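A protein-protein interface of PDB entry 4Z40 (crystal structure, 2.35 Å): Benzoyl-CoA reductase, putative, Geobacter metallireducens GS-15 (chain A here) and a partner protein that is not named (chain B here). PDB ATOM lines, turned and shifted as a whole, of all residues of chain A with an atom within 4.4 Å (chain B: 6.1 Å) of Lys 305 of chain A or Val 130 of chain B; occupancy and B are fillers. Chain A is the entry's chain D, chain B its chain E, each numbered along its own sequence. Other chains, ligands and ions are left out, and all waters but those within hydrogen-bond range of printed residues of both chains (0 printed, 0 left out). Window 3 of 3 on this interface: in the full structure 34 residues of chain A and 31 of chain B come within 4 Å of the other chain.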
ATOM      1  N   LYS A 253     -29.387  22.695 -29.315  1.00  0.00           N
ATOM      2  CA  LYS A 253     -29.620  23.081 -27.927  1.00  0.00           C
ATOM      3  C   LYS A 253     -31.023  22.673 -27.497  1.00  0.00           C
ATOM      4  O   LYS A 253     -31.604  21.761 -28.078  1.00  0.00           O
ATOM      5  CB  LYS A 253     -29.378  24.576 -27.761  1.00  0.00           C
ATOM      6  CG  LYS A 253     -28.099  24.974 -28.474  1.00  0.00           C
ATOM      7  CD  LYS A 253     -27.581  26.339 -28.113  1.00  0.00           C
ATOM      8  CE  LYS A 253     -26.154  26.486 -28.646  1.00  0.00           C
ATOM      9  NZ  LYS A 253     -25.568  27.823 -28.370  1.00  0.00           N
ATOM     10  N   LEU A 296     -21.337  21.085 -27.733  1.00  0.00           N
ATOM     11  CA  LEU A 296     -21.732  22.147 -28.641  1.00  0.00           C
ATOM     12  C   LEU A 296     -20.483  22.880 -29.086  1.00  0.00           C
ATOM     13  O   LEU A 296     -19.740  23.374 -28.258  1.00  0.00           O
ATOM     14  CB  LEU A 296     -22.713  23.107 -27.962  1.00  0.00           C
ATOM     15  CG  LEU A 296     -24.039  22.492 -27.512  1.00  0.00           C
ATOM     16  CD1 LEU A 296     -24.727  23.381 -26.468  1.00  0.00           C
ATOM     17  CD2 LEU A 296     -24.955  22.252 -28.737  1.00  0.00           C
ATOM     18  N   ILE A 297     -20.247  22.946 -30.392  1.00  0.00           N
ATOM     19  CA  ILE A 297     -18.990  23.493 -30.910  1.00  0.00           C
ATOM     20  C   ILE A 297     -19.223  24.565 -31.973  1.00  0.00           C
ATOM     21  O   ILE A 297     -20.245  24.560 -32.658  1.00  0.00           O
ATOM     22  CB  ILE A 297     -18.101  22.380 -31.502  1.00  0.00           C
ATOM     23  CG1 ILE A 297     -18.807  21.680 -32.666  1.00  0.00           C
ATOM     24  CG2 ILE A 297     -17.736  21.373 -30.432  1.00  0.00           C
ATOM     25  CD1 ILE A 297     -17.912  20.713 -33.416  1.00  0.00           C
ATOM     26  N   SER A 298     -18.256  25.466 -32.111  1.00  0.00           N
ATOM     27  CA  SER A 298     -18.376  26.609 -33.011  1.00  0.00           C
ATOM     28  C   SER A 298     -17.633  26.484 -34.340  1.00  0.00           C
ATOM     29  O   SER A 298     -16.660  25.724 -34.456  1.00  0.00           O
ATOM     30  CB  SER A 298     -17.857  27.859 -32.304  1.00  0.00           C
ATOM     31  OG  SER A 298     -18.668  28.228 -31.205  1.00  0.00           O
ATOM     32  N   PRO A 303     -18.646  32.650 -31.155  1.00  0.00           N
ATOM     33  CA  PRO A 303     -19.027  32.131 -29.843  1.00  0.00           C
ATOM     34  C   PRO A 303     -20.381  31.426 -29.803  1.00  0.00           C
ATOM     35  O   PRO A 303     -20.764  30.950 -28.738  1.00  0.00           O
ATOM     36  CB  PRO A 303     -19.069  33.394 -28.992  1.00  0.00           C
ATOM     37  CG  PRO A 303     -19.546  34.432 -29.943  1.00  0.00           C
ATOM     38  CD  PRO A 303     -18.951  34.083 -31.284  1.00  0.00           C
ATOM     39  N   MET A 304     -21.089  31.348 -30.925  1.00  0.00           N
ATOM     40  CA  MET A 304     -22.476  30.879 -30.908  1.00  0.00           C
ATOM     41  C   MET A 304     -22.653  29.358 -30.796  1.00  0.00           C
ATOM     42  O   MET A 304     -23.739  28.895 -30.461  1.00  0.00           O
ATOM     43  CB  MET A 304     -23.200  31.377 -32.157  1.00  0.00           C
ATOM     44  CG  MET A 304     -23.273  32.890 -32.282  1.00  0.00           C
ATOM     45  SD  MET A 304     -23.847  33.717 -30.777  1.00  0.00           S
ATOM     46  CE  MET A 304     -25.426  32.918 -30.504  1.00  0.00           C
ATOM     47  N   LYS A 305     -21.587  28.599 -31.061  1.00  0.00           N
ATOM     48  CA  LYS A 305     -21.578  27.123 -31.020  1.00  0.00           C
ATOM     49  C   LYS A 305     -22.892  26.441 -31.405  1.00  0.00           C
ATOM     50  O   LYS A 305     -23.510  25.746 -30.588  1.00  0.00           O
ATOM     51  CB  LYS A 305     -21.135  26.633 -29.632  1.00  0.00           C
ATOM     52  CG  LYS A 305     -21.853  27.263 -28.451  1.00  0.00           C
ATOM     53  CD  LYS A 305     -21.228  26.851 -27.141  1.00  0.00           C
ATOM     54  CE  LYS A 305     -21.998  27.432 -25.985  1.00  0.00           C
ATOM     55  NZ  LYS A 305     -21.463  26.956 -24.673  1.00  0.00           N
ATOM     56  N   CYS A 306     -23.289  26.630 -32.662  1.00  0.00           N
ATOM     57  CA  CYS A 306     -24.529  26.082 -33.198  1.00  0.00           C
ATOM     58  C   CYS A 306     -24.480  24.569 -33.406  1.00  0.00           C
ATOM     59  O   CYS A 306     -25.489  23.876 -33.242  1.00  0.00           O
ATOM     60  CB  CYS A 306     -24.863  26.770 -34.525  1.00  0.00           C
ATOM     61  SG  CYS A 306     -25.041  28.558 -34.361  1.00  0.00           S
ATOM     62  N   GLY A 307     -23.310  24.062 -33.772  1.00  0.00           N
ATOM     63  CA  GLY A 307     -23.152  22.653 -34.083  1.00  0.00           C
ATOM     64  C   GLY A 307     -23.034  21.781 -32.855  1.00  0.00           C
ATOM     65  O   GLY A 307     -22.807  22.268 -31.754  1.00  0.00           O
ATOM     66  N   LYS B  19     -15.380  23.930 -21.124  1.00  0.00           N
ATOM     67  CA  LYS B  19     -16.207  25.002 -21.662  1.00  0.00           C
ATOM     68  C   LYS B  19     -15.820  25.373 -23.086  1.00  0.00           C
ATOM     69  O   LYS B  19     -16.628  25.971 -23.816  1.00  0.00           O
ATOM     70  CB  LYS B  19     -16.117  26.249 -20.786  1.00  0.00           C
ATOM     71  CG  LYS B  19     -16.857  26.172 -19.463  1.00  0.00           C
ATOM     72  CD  LYS B  19     -16.511  27.383 -18.608  1.00  0.00           C
ATOM     73  CE  LYS B  19     -17.696  27.843 -17.776  1.00  0.00           C
ATOM     74  NZ  LYS B  19     -17.461  29.183 -17.152  1.00  0.00           N
ATOM     75  N   CYS B  20     -14.601  25.031 -23.487  1.00  0.00           N
ATOM     76  CA  CYS B  20     -14.101  25.453 -24.795  1.00  0.00           C
ATOM     77  C   CYS B  20     -14.930  24.885 -25.936  1.00  0.00           C
ATOM     78  O   CYS B  20     -15.329  23.723 -25.905  1.00  0.00           O
ATOM     79  CB  CYS B  20     -12.645  25.049 -24.982  1.00  0.00           C
ATOM     80  SG  CYS B  20     -11.953  25.605 -26.542  1.00  0.00           S
ATOM     81  N   ASN B  21     -15.198  25.702 -26.945  1.00  0.00           N
ATOM     82  CA  ASN B  21     -15.928  25.195 -28.110  1.00  0.00           C
ATOM     83  C   ASN B  21     -15.037  25.072 -29.344  1.00  0.00           C
ATOM     84  O   ASN B  21     -15.490  24.627 -30.393  1.00  0.00           O
ATOM     85  CB  ASN B  21     -17.146  26.062 -28.415  1.00  0.00           C
ATOM     86  CG  ASN B  21     -16.837  27.544 -28.408  1.00  0.00           C
ATOM     87  OD1 ASN B  21     -16.110  28.044 -29.262  1.00  0.00           O
ATOM     88  ND2 ASN B  21     -17.419  28.261 -27.455  1.00  0.00           N
ATOM     89  N   TRP B 127     -11.891  37.944 -25.602  1.00  0.00           N
ATOM     90  CA  TRP B 127     -12.587  37.514 -26.800  1.00  0.00           C
ATOM     91  C   TRP B 127     -13.186  36.127 -26.654  1.00  0.00           C
ATOM     92  O   TRP B 127     -13.896  35.652 -27.548  1.00  0.00           O
ATOM     93  CB  TRP B 127     -11.646  37.554 -28.003  1.00  0.00           C
ATOM     94  CG  TRP B 127     -11.594  38.895 -28.621  1.00  0.00           C
ATOM     95  CD1 TRP B 127     -11.511  40.089 -27.973  1.00  0.00           C
ATOM     96  CD2 TRP B 127     -11.673  39.197 -30.016  1.00  0.00           C
ATOM     97  NE1 TRP B 127     -11.510  41.121 -28.880  1.00  0.00           N
ATOM     98  CE2 TRP B 127     -11.611  40.599 -30.143  1.00  0.00           C
ATOM     99  CE3 TRP B 127     -11.778  38.420 -31.173  1.00  0.00           C
ATOM    100  CZ2 TRP B 127     -11.656  41.241 -31.381  1.00  0.00           C
ATOM    101  CZ3 TRP B 127     -11.824  39.061 -32.401  1.00  0.00           C
ATOM    102  CH2 TRP B 127     -11.761  40.455 -32.494  1.00  0.00           C
ATOM    103  N   CYS B 128     -12.910  35.473 -25.533  1.00  0.00           N
ATOM    104  CA  CYS B 128     -13.516  34.174 -25.277  1.00  0.00           C
ATOM    105  C   CYS B 128     -14.849  34.369 -24.563  1.00  0.00           C
ATOM    106  O   CYS B 128     -14.924  34.291 -23.334  1.00  0.00           O
ATOM    107  CB  CYS B 128     -12.579  33.288 -24.460  1.00  0.00           C
ATOM    108  SG  CYS B 128     -13.223  31.642 -24.168  1.00  0.00           S
ATOM    109  N   LEU B 129     -15.903  34.627 -25.343  1.00  0.00           N
ATOM    110  CA  LEU B 129     -17.191  35.020 -24.785  1.00  0.00           C
ATOM    111  C   LEU B 129     -17.875  33.936 -23.942  1.00  0.00           C
ATOM    112  O   LEU B 129     -18.669  34.253 -23.057  1.00  0.00           O
ATOM    113  CB  LEU B 129     -18.133  35.481 -25.907  1.00  0.00           C
ATOM    114  CG  LEU B 129     -18.251  36.995 -26.114  1.00  0.00           C
ATOM    115  CD1 LEU B 129     -16.943  37.576 -26.614  1.00  0.00           C
ATOM    116  CD2 LEU B 129     -19.400  37.349 -27.063  1.00  0.00           C
ATOM    117  N   VAL B 130     -17.588  32.669 -24.210  1.00  0.00           N
ATOM    118  CA  VAL B 130     -18.114  31.588 -23.377  1.00  0.00           C
ATOM    119  C   VAL B 130     -17.403  31.542 -22.008  1.00  0.00           C
ATOM    120  O   VAL B 130     -17.875  30.897 -21.072  1.00  0.00           O
ATOM    121  CB  VAL B 130     -17.982  30.215 -24.085  1.00  0.00           C
ATOM    122  CG1 VAL B 130     -16.517  29.781 -24.167  1.00  0.00           C
ATOM    123  CG2 VAL B 130     -18.822  29.145 -23.384  1.00  0.00           C
ATOM    124  N   GLY B 131     -16.268  32.229 -21.899  1.00  0.00           N
ATOM    125  CA  GLY B 131     -15.567  32.365 -20.632  1.00  0.00           C
ATOM    126  C   GLY B 131     -14.737  31.174 -20.169  1.00  0.00           C
ATOM    127  O   GLY B 131     -14.769  30.812 -18.993  1.00  0.00           O
ATOM    128  N   ALA B 132     -13.978  30.573 -21.074  1.00  0.00           N
ATOM    129  CA  ALA B 132     -13.182  29.402 -20.735  1.00  0.00           C
ATOM    130  C   ALA B 132     -11.822  29.813 -20.165  1.00  0.00           C
ATOM    131  O   ALA B 132     -11.066  28.981 -19.651  1.00  0.00           O
ATOM    132  CB  ALA B 132     -13.002  28.510 -21.966  1.00  0.00           C
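Of the 9 printed residues of chain B, 3 touch a printed residue of chain A.
Of the 9 printed residues of chain A, 5 touch a printed residue of chain B.
Hydrophobic or aromatic side chains of chain A within 4 Å of the printed part of chain B: Ile 297 and Pro 303.
Among the printed residues, 5 pairs touch across the chains.
Among the printed residues, no Asp or Glu carboxylate lies within 4 Å of a Lys or Arg side-chain nitrogen of the other chain.
The side-chain amide oxygen of Asn 21 of chain B sits at hydrogen-bond distance from the side-chain hydroxyl of Ser 298 of chain A, at 3.2 Å.
The backbone NH (N) of Ile 297 of chain A is in hydrogen-bond range of the backbone carbonyl oxygen (O) of Gly 307 of chain A (3.0 Å).
The side-chain hydroxyl (OG) of Ser 298 of chain A is in hydrogen-bond range of the backbone NH (N) of Lys 305 of chain A (2.9 Å).
Of chain B, only Val 130 (3.7 Å) comes within 4 Å of Lys 305 of chain A.
Of the printed residues of chain B, Leu 296 of chain A touches Asn 21.
Of the printed residues of chain B, Pro 303 of chain A touches Leu 129 (3.8 Å).
Of the printed residues of chain A, Leu 129 of chain B touches Pro 303.
The nearest residue of chain B that does not touch Lys 305 of chain A is Asn 21 of chain B (4.1 Å).
The nearest printed residue of chain A that does not touch Val 130 of chain B is Pro 303 of chain A (5.1 Å).
The nearest printed residue of chain A that does not touch Leu 129 of chain B is Met 304 of chain A (6.8 Å).
Among the printed residues, merely in contact across the chains: Leu 296 of chain A with Asn 21 of chain B, Ile 297 of chain A with Asn 21 of chain B, Pro 303 of chain A with Leu 129 of chain B and Lys 305 of chain A with Val 130 of chain B.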
